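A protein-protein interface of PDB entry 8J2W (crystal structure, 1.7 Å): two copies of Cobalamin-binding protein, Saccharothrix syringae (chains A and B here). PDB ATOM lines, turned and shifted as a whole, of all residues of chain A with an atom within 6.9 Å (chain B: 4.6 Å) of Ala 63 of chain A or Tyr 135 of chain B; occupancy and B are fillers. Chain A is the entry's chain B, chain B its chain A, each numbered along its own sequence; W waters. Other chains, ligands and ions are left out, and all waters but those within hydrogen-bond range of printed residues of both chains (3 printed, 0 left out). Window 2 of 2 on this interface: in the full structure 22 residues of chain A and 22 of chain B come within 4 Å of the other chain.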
ATOM      1  N   LEU A  14      -9.502   6.797  -1.500  1.00  0.00           N
ATOM      2  CA  LEU A  14     -10.355   5.649  -1.277  1.00  0.00           C
ATOM      3  C   LEU A  14      -9.677   4.610  -0.388  1.00  0.00           C
ATOM      4  O   LEU A  14     -10.312   4.057   0.517  1.00  0.00           O
ATOM      5  CB  LEU A  14     -10.784   5.017  -2.625  1.00  0.00           C
ATOM      6  CG  LEU A  14     -11.701   5.897  -3.517  1.00  0.00           C
ATOM      7  CD1 LEU A  14     -12.092   5.170  -4.746  1.00  0.00           C
ATOM      8  CD2 LEU A  14     -12.916   6.351  -2.736  1.00  0.00           C
ATOM      9  N   ALA A  15      -8.397   4.343  -0.650  1.00  0.00           N
ATOM     10  CA  ALA A  15      -7.625   3.392   0.134  1.00  0.00           C
ATOM     11  C   ALA A  15      -7.438   3.864   1.578  1.00  0.00           C
ATOM     12  O   ALA A  15      -7.301   3.046   2.494  1.00  0.00           O
ATOM     13  CB  ALA A  15      -6.257   3.155  -0.515  1.00  0.00           C
ATOM     14  N   GLU A  16      -7.390   5.190   1.764  1.00  0.00           N
ATOM     15  CA  GLU A  16      -7.263   5.782   3.086  1.00  0.00           C
ATOM     16  C   GLU A  16      -8.604   5.918   3.803  1.00  0.00           C
ATOM     17  O   GLU A  16      -8.638   6.212   4.994  1.00  0.00           O
ATOM     18  CB  GLU A  16      -6.610   7.187   2.989  1.00  0.00           C
ATOM     19  CG  GLU A  16      -5.120   7.136   2.696  1.00  0.00           C
ATOM     20  CD  GLU A  16      -4.296   6.569   3.839  1.00  0.00           C
ATOM     21  OE1 GLU A  16      -4.842   6.451   4.964  1.00  0.00           O
ATOM     22  OE2 GLU A  16      -3.117   6.220   3.599  1.00  0.00           O
ATOM     23  N   GLY A  17      -9.707   5.707   3.086  1.00  0.00           N
ATOM     24  CA  GLY A  17     -11.030   5.914   3.652  1.00  0.00           C
ATOM     25  C   GLY A  17     -11.314   7.375   3.996  1.00  0.00           C
ATOM     26  O   GLY A  17     -11.939   7.659   5.017  1.00  0.00           O
ATOM     27  N   TRP A  60      -7.664  -6.738  -0.816  1.00  0.00           N
ATOM     28  CA  TRP A  60      -8.507  -5.875  -0.001  1.00  0.00           C
ATOM     29  C   TRP A  60      -9.614  -6.655   0.708  1.00  0.00           C
ATOM     30  O   TRP A  60     -10.196  -7.577   0.142  1.00  0.00           O
ATOM     31  CB  TRP A  60      -9.170  -4.789  -0.850  1.00  0.00           C
ATOM     32  CG  TRP A  60      -8.376  -3.536  -1.019  1.00  0.00           C
ATOM     33  CD1 TRP A  60      -7.017  -3.399  -1.060  1.00  0.00           C
ATOM     34  CD2 TRP A  60      -8.923  -2.233  -1.224  1.00  0.00           C
ATOM     35  NE1 TRP A  60      -6.684  -2.068  -1.222  1.00  0.00           N
ATOM     36  CE2 TRP A  60      -7.845  -1.336  -1.355  1.00  0.00           C
ATOM     37  CE3 TRP A  60     -10.230  -1.733  -1.285  1.00  0.00           C
ATOM     38  CZ2 TRP A  60      -8.038   0.035  -1.551  1.00  0.00           C
ATOM     39  CZ3 TRP A  60     -10.413  -0.376  -1.465  1.00  0.00           C
ATOM     40  CH2 TRP A  60      -9.327   0.485  -1.609  1.00  0.00           C
ATOM     41  N   SER A  61      -9.909  -6.257   1.943  1.00  0.00           N
ATOM     42  CA  SER A  61     -11.019  -6.807   2.696  1.00  0.00           C
ATOM     43  C   SER A  61     -12.351  -6.156   2.303  1.00  0.00           C
ATOM     44  O   SER A  61     -12.407  -5.141   1.612  1.00  0.00           O
ATOM     45  CB  SER A  61     -10.790  -6.611   4.191  1.00  0.00           C
ATOM     46  OG  SER A  61     -11.081  -5.276   4.572  1.00  0.00           O
ATOM     47  N   VAL A  62     -13.427  -6.744   2.806  1.00  0.00           N
ATOM     48  CA  VAL A  62     -14.761  -6.199   2.639  1.00  0.00           C
ATOM     49  C   VAL A  62     -14.873  -4.830   3.307  1.00  0.00           C
ATOM     50  O   VAL A  62     -15.564  -3.942   2.788  1.00  0.00           O
ATOM     51  CB  VAL A  62     -15.825  -7.182   3.183  1.00  0.00           C
ATOM     52  CG1 VAL A  62     -17.191  -6.526   3.194  1.00  0.00           C
ATOM     53  CG2 VAL A  62     -15.834  -8.482   2.384  1.00  0.00           C
ATOM     54  N   ALA A  63     -14.219  -4.675   4.474  1.00  0.00           N
ATOM     55  CA  ALA A  63     -14.216  -3.399   5.153  1.00  0.00           C
ATOM     56  C   ALA A  63     -13.565  -2.320   4.279  1.00  0.00           C
ATOM     57  O   ALA A  63     -14.112  -1.231   4.170  1.00  0.00           O
ATOM     58  CB  ALA A  63     -13.529  -3.477   6.492  1.00  0.00           C
ATOM     59  N   GLN A  64     -12.415  -2.637   3.660  1.00  0.00           N
ATOM     60  CA  GLN A  64     -11.724  -1.678   2.800  1.00  0.00           C
ATOM     61  C   GLN A  64     -12.566  -1.278   1.597  1.00  0.00           C
ATOM     62  O   GLN A  64     -12.703  -0.090   1.302  1.00  0.00           O
ATOM     63  CB  GLN A  64     -10.355  -2.236   2.345  1.00  0.00           C
ATOM     64  CG  GLN A  64      -9.378  -2.455   3.487  1.00  0.00           C
ATOM     65  CD  GLN A  64      -8.099  -3.102   3.014  1.00  0.00           C
ATOM     66  OE1 GLN A  64      -7.980  -4.345   2.980  1.00  0.00           O
ATOM     67  NE2 GLN A  64      -7.154  -2.262   2.576  1.00  0.00           N
ATOM     68  N   GLU A  65     -13.142  -2.268   0.907  1.00  0.00           N
ATOM     69  CA  GLU A  65     -14.060  -2.001  -0.188  1.00  0.00           C
ATOM     70  C   GLU A  65     -15.264  -1.162   0.245  1.00  0.00           C
ATOM     71  O   GLU A  65     -15.555  -0.158  -0.388  1.00  0.00           O
ATOM     72  CB  GLU A  65     -14.523  -3.284  -0.871  1.00  0.00           C
ATOM     73  CG  GLU A  65     -15.670  -3.059  -1.846  1.00  0.00           C
ATOM     74  CD  GLU A  65     -17.039  -3.034  -1.204  1.00  0.00           C
ATOM     75  OE1 GLU A  65     -17.301  -3.971  -0.409  1.00  0.00           O
ATOM     76  OE2 GLU A  65     -17.836  -2.092  -1.479  1.00  0.00           O
ATOM     77  N   HIS A  66     -15.918  -1.540   1.357  1.00  0.00           N
ATOM     78  CA  HIS A  66     -17.076  -0.805   1.842  1.00  0.00           C
ATOM     79  C   HIS A  66     -16.746   0.666   2.084  1.00  0.00           C
ATOM     80  O   HIS A  66     -17.536   1.545   1.724  1.00  0.00           O
ATOM     81  CB  HIS A  66     -17.646  -1.415   3.128  1.00  0.00           C
ATOM     82  CG  HIS A  66     -18.599  -2.550   2.938  1.00  0.00           C
ATOM     83  ND1 HIS A  66     -18.562  -3.503   1.938  1.00  0.00           N
ATOM     84  CD2 HIS A  66     -19.637  -2.887   3.732  1.00  0.00           C
ATOM     85  CE1 HIS A  66     -19.544  -4.385   2.120  1.00  0.00           C
ATOM     86  NE2 HIS A  66     -20.211  -4.040   3.211  1.00  0.00           N
ATOM     87  N   ALA A  67     -15.589   0.936   2.691  1.00  0.00           N
ATOM     88  CA  ALA A  67     -15.191   2.304   2.980  1.00  0.00           C
ATOM     89  C   ALA A  67     -15.067   3.103   1.682  1.00  0.00           C
ATOM     90  O   ALA A  67     -15.558   4.225   1.587  1.00  0.00           O
ATOM     91  CB  ALA A  67     -13.891   2.334   3.747  1.00  0.00           C
ATOM     92  N   ALA A  68     -14.413   2.494   0.696  1.00  0.00           N
ATOM     93  CA  ALA A  68     -14.184   3.123  -0.595  1.00  0.00           C
ATOM     94  C   ALA A  68     -15.494   3.377  -1.351  1.00  0.00           C
ATOM     95  O   ALA A  68     -15.736   4.475  -1.836  1.00  0.00           O
ATOM     96  CB  ALA A  68     -13.278   2.250  -1.423  1.00  0.00           C
ATOM     97  N   VAL B  93     -15.035   4.352  13.691  1.00  0.00           N
ATOM     98  CA  VAL B  93     -15.483   3.528  12.589  1.00  0.00           C
ATOM     99  C   VAL B  93     -16.955   3.174  12.828  1.00  0.00           C
ATOM    100  O   VAL B  93     -17.302   2.651  13.888  1.00  0.00           O
ATOM    101  CB  VAL B  93     -14.612   2.256  12.434  1.00  0.00           C
ATOM    102  CG1 VAL B  93     -15.198   1.293  11.410  1.00  0.00           C
ATOM    103  CG2 VAL B  93     -13.171   2.580  12.086  1.00  0.00           C
ATOM    104  N   THR B 121     -14.938   7.023   9.700  1.00  0.00           N
ATOM    105  CA  THR B 121     -14.918   6.165   8.522  1.00  0.00           C
ATOM    106  C   THR B 121     -16.206   5.347   8.499  1.00  0.00           C
ATOM    107  O   THR B 121     -16.447   4.545   9.407  1.00  0.00           O
ATOM    108  CB  THR B 121     -13.721   5.232   8.480  1.00  0.00           C
ATOM    109  OG1 THR B 121     -12.530   5.960   8.713  1.00  0.00           O
ATOM    110  CG2 THR B 121     -13.621   4.507   7.158  1.00  0.00           C
ATOM    111  N   LEU B 123     -18.533   2.513   7.115  1.00  0.00           N
ATOM    112  CA  LEU B 123     -18.482   1.255   6.393  1.00  0.00           C
ATOM    113  C   LEU B 123     -19.868   0.815   5.946  1.00  0.00           C
ATOM    114  O   LEU B 123     -19.975   0.071   4.981  1.00  0.00           O
ATOM    115  CB  LEU B 123     -17.854   0.160   7.227  1.00  0.00           C
ATOM    116  CG  LEU B 123     -16.467   0.443   7.747  1.00  0.00           C
ATOM    117  CD1 LEU B 123     -15.878  -0.776   8.436  1.00  0.00           C
ATOM    118  CD2 LEU B 123     -15.530   0.939   6.650  1.00  0.00           C
ATOM    119  N   VAL B 127     -21.083  -5.682   7.329  1.00  0.00           N
ATOM    120  CA  VAL B 127     -19.646  -5.916   7.405  1.00  0.00           C
ATOM    121  C   VAL B 127     -19.396  -7.191   8.212  1.00  0.00           C
ATOM    122  O   VAL B 127     -19.641  -7.220   9.417  1.00  0.00           O
ATOM    123  CB  VAL B 127     -18.877  -4.760   8.066  1.00  0.00           C
ATOM    124  CG1 VAL B 127     -17.368  -5.005   7.941  1.00  0.00           C
ATOM    125  CG2 VAL B 127     -19.280  -3.414   7.507  1.00  0.00           C
ATOM    126  N   HIS B 131     -13.880  -9.546   8.668  1.00  0.00           N
ATOM    127  CA  HIS B 131     -13.281  -8.434   7.939  1.00  0.00           C
ATOM    128  C   HIS B 131     -13.190  -7.181   8.813  1.00  0.00           C
ATOM    129  O   HIS B 131     -12.236  -6.398   8.697  1.00  0.00           O
ATOM    130  CB  HIS B 131     -14.036  -8.188   6.633  1.00  0.00           C
ATOM    131  CG  HIS B 131     -13.919  -9.308   5.657  1.00  0.00           C
ATOM    132  ND1 HIS B 131     -13.097  -9.263   4.553  1.00  0.00           N
ATOM    133  CD2 HIS B 131     -14.498 -10.521   5.632  1.00  0.00           C
ATOM    134  CE1 HIS B 131     -13.189 -10.410   3.881  1.00  0.00           C
ATOM    135  NE2 HIS B 131     -14.037 -11.190   4.519  1.00  0.00           N
ATOM    136  N   LEU B 132     -14.185  -6.971   9.679  1.00  0.00           N
ATOM    137  CA  LEU B 132     -14.197  -5.807  10.554  1.00  0.00           C
ATOM    138  C   LEU B 132     -13.076  -5.857  11.588  1.00  0.00           C
ATOM    139  O   LEU B 132     -12.431  -4.844  11.861  1.00  0.00           O
ATOM    140  CB  LEU B 132     -15.577  -5.687  11.264  1.00  0.00           C
ATOM    141  CG  LEU B 132     -15.758  -4.521  12.226  1.00  0.00           C
ATOM    142  CD1 LEU B 132     -15.517  -3.159  11.518  1.00  0.00           C
ATOM    143  CD2 LEU B 132     -17.123  -4.552  12.861  1.00  0.00           C
ATOM    144  N   VAL B 133     -12.866  -7.035  12.198  1.00  0.00           N
ATOM    145  CA  VAL B 133     -11.857  -7.164  13.238  1.00  0.00           C
ATOM    146  C   VAL B 133     -10.466  -6.775  12.732  1.00  0.00           C
ATOM    147  O   VAL B 133      -9.819  -5.905  13.324  1.00  0.00           O
ATOM    148  CB  VAL B 133     -11.917  -8.587  13.859  1.00  0.00           C
ATOM    149  CG1 VAL B 133     -10.625  -8.940  14.608  1.00  0.00           C
ATOM    150  CG2 VAL B 133     -13.134  -8.698  14.752  1.00  0.00           C
ATOM    151  N   PRO B 134      -9.950  -7.349  11.617  1.00  0.00           N
ATOM    152  CA  PRO B 134      -8.661  -6.885  11.087  1.00  0.00           C
ATOM    153  C   PRO B 134      -8.614  -5.403  10.709  1.00  0.00           C
ATOM    154  O   PRO B 134      -7.559  -4.794  10.814  1.00  0.00           O
ATOM    155  CB  PRO B 134      -8.378  -7.797   9.880  1.00  0.00           C
ATOM    156  CG  PRO B 134      -9.606  -8.641   9.701  1.00  0.00           C
ATOM    157  CD  PRO B 134     -10.469  -8.538  10.920  1.00  0.00           C
ATOM    158  N   TYR B 135      -9.743  -4.825  10.282  1.00  0.00           N
ATOM    159  CA  TYR B 135      -9.804  -3.394  10.008  1.00  0.00           C
ATOM    160  C   TYR B 135      -9.568  -2.580  11.287  1.00  0.00           C
ATOM    161  O   TYR B 135      -8.837  -1.586  11.271  1.00  0.00           O
ATOM    162  CB  TYR B 135     -11.155  -3.026   9.376  1.00  0.00           C
ATOM    163  CG  TYR B 135     -11.181  -1.659   8.737  1.00  0.00           C
ATOM    164  CD1 TYR B 135     -10.643  -1.448   7.476  1.00  0.00           C
ATOM    165  CD2 TYR B 135     -11.751  -0.578   9.390  1.00  0.00           C
ATOM    166  CE1 TYR B 135     -10.682  -0.192   6.881  1.00  0.00           C
ATOM    167  CE2 TYR B 135     -11.772   0.684   8.818  1.00  0.00           C
ATOM    168  CZ  TYR B 135     -11.246   0.872   7.555  1.00  0.00           C
ATOM    169  OH  TYR B 135     -11.305   2.141   6.999  1.00  0.00           O
ATOM    170  N   LEU B 136     -10.178  -3.014  12.399  1.00  0.00           N
ATOM    171  CA  LEU B 136      -9.985  -2.360  13.684  1.00  0.00           C
ATOM    172  C   LEU B 136      -8.555  -2.539  14.197  1.00  0.00           C
ATOM    173  O   LEU B 136      -7.980  -1.630  14.797  1.00  0.00           O
ATOM    174  CB  LEU B 136     -10.981  -2.896  14.753  1.00  0.00           C
ATOM    175  CG  LEU B 136     -12.452  -2.712  14.427  1.00  0.00           C
ATOM    176  CD1 LEU B 136     -13.340  -3.213  15.595  1.00  0.00           C
ATOM    177  CD2 LEU B 136     -12.753  -1.290  14.118  1.00  0.00           C
ATOM    178  N   GLU B 137      -7.978  -3.720  13.955  1.00  0.00           N
ATOM    179  CA  GLU B 137      -6.596  -3.987  14.333  1.00  0.00           C
ATOM    180  C   GLU B 137      -5.629  -3.127  13.519  1.00  0.00           C
ATOM    181  O   GLU B 137      -4.598  -2.666  14.024  1.00  0.00           O
ATOM    182  CB  GLU B 137      -6.281  -5.475  14.145  1.00  0.00           C
ATOM    183  CG  GLU B 137      -7.015  -6.380  15.128  1.00  0.00           C
ATOM    184  CD  GLU B 137      -6.935  -7.883  14.858  1.00  0.00           C
ATOM    185  OE1 GLU B 137      -6.672  -8.277  13.694  1.00  0.00           O
ATOM    186  OE2 GLU B 137      -7.125  -8.669  15.820  1.00  0.00           O
ATOM    187  N   GLU B 138      -5.958  -2.930  12.239  1.00  0.00           N
ATOM    188  CA  GLU B 138      -5.146  -2.128  11.336  1.00  0.00           C
ATOM    189  C   GLU B 138      -5.106  -0.643  11.703  1.00  0.00           C
ATOM    190  O   GLU B 138      -4.061  -0.020  11.548  1.00  0.00           O
ATOM    191  CB  GLU B 138      -5.707  -2.266   9.904  1.00  0.00           C
ATOM    192  CG  GLU B 138      -4.880  -1.619   8.817  1.00  0.00           C
ATOM    193  CD  GLU B 138      -3.552  -2.307   8.606  1.00  0.00           C
ATOM    194  OE1 GLU B 138      -3.529  -3.528   8.334  1.00  0.00           O
ATOM    195  OE2 GLU B 138      -2.526  -1.622   8.751  1.00  0.00           O
ATOM    196  N   HIS B 139      -6.243  -0.080  12.148  1.00  0.00           N
ATOM    197  CA  HIS B 139      -6.383   1.368  12.276  1.00  0.00           C
ATOM    198  C   HIS B 139      -6.559   1.849  13.720  1.00  0.00           C
ATOM    199  O   HIS B 139      -6.435   3.042  13.982  1.00  0.00           O
ATOM    200  CB  HIS B 139      -7.547   1.855  11.409  1.00  0.00           C
ATOM    201  CG  HIS B 139      -7.323   1.612   9.959  1.00  0.00           C
ATOM    202  ND1 HIS B 139      -6.335   2.266   9.255  1.00  0.00           N
ATOM    203  CD2 HIS B 139      -7.943   0.785   9.094  1.00  0.00           C
ATOM    204  CE1 HIS B 139      -6.373   1.854   7.989  1.00  0.00           C
ATOM    205  NE2 HIS B 139      -7.317   0.949   7.874  1.00  0.00           N
HETATM  206  O   HOH W   1     -11.548   8.563   8.035  1.00  0.00           O
HETATM  207  O   HOH W   2      -7.786   2.871   5.213  1.00  0.00           O
HETATM  208  O   HOH W   3     -10.054  -5.417   6.989  1.00  0.00           O
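N of Val 62 of chain A lies within hydrogen-bond range of ND1 of His 131 of chain B, at 3.1 Å.
O of Val 62 of chain A lies within hydrogen-bond range of ND1 of His 66 of chain A, 3.1 Å away. N of Ser 61 of chain A lies within hydrogen-bond range of OE1 of Gln 64 of chain A (2.9 Å). ND1 of His 66 of chain A is in hydrogen-bond range of OE1 of Glu 65 of chain A (2.7 Å). The side-chain hydroxyl (OG) of Ser 61 of chain A sits at hydrogen-bond distance from the backbone NH (N) of Ala 63 of chain A (3.2 Å).
Among the printed residues, merely in contact across the chains: His 66 of chain A with Leu 123 of chain B (3.2 Å), Ser 61 of chain A with His 131 of chain B (3.5 Å), Ala 63 of chain A with Leu 123 of chain B (3.6 Å), Ala 67 of chain A with Leu 123 of chain B (3.6 Å), Ala 63 of chain A with Tyr 135 of chain B (3.7 Å), His 66 of chain A with Val 127 of chain B (3.8 Å) and Ala 63 of chain A with His 131 of chain B (3.9 Å).
Ala 63 of chain A touches just these residues of chain B: Leu 123, His 131 and Tyr 135. Printed residues of chain B within 4 Å of Val 62 of chain A: His 131 (3.1 Å). Printed residues of chain B within 4 Å of Ala 67 of chain A: Leu 123 (3.6 Å). Of the printed residues of chain B, His 66 of chain A touches Leu 123 (3.2 Å) and Val 127 (3.8 Å). Printed residues of chain A within 4 Å of Val 127 of chain B: His 66. Printed residues of chain B within 4 Å of Ser 61 of chain A: His 131. Pro 134 of chain B touches none of the printed residues of chain A. Ala 15 of chain A touches none of the printed residues of chain B. The nearest residue of chain B that does not touch Ala 63 of chain A is Val 127 of chain B (4.4 Å). The nearest printed residue of chain A that does not touch Val 127 of chain B is Ala 63 of chain A (4.4 Å).
Printed residues of chain B that touch a printed residue of chain A: Leu 123, Val 127, His 131 and Tyr 135. Hydrophobic or aromatic side chains of chain A that line the printed part of chain B: Val 62, Ala 63, His 66 and Ala 67. Among the printed residues, no Asp or Glu carboxylate lies within 4 Å of a Lys or Arg side-chain nitrogen of the other chain.
No position is printed for both chains. Of the 8 pairs that touch across the chains among the printed residues, none has its exchanged pair printed and touching as well.
Water W3 lies within hydrogen-bond range of the side-chain hydroxyl (OG) of Ser 61 of chain A, the backbone carbonyl oxygen (O) of His 131 of chain B and the backbone NH (N) of Tyr 135 of chain B. Water W2 lies within hydrogen-bond range of O of Ala 15 of chain A, NE2 of His 139 of chain B and O of Glu 16 of chain A. Water W1 lies within hydrogen-bond range of OG1 of Thr 121 of chain B (2.9 Å) and O of Gly 17 of chain A (3.2 Å).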
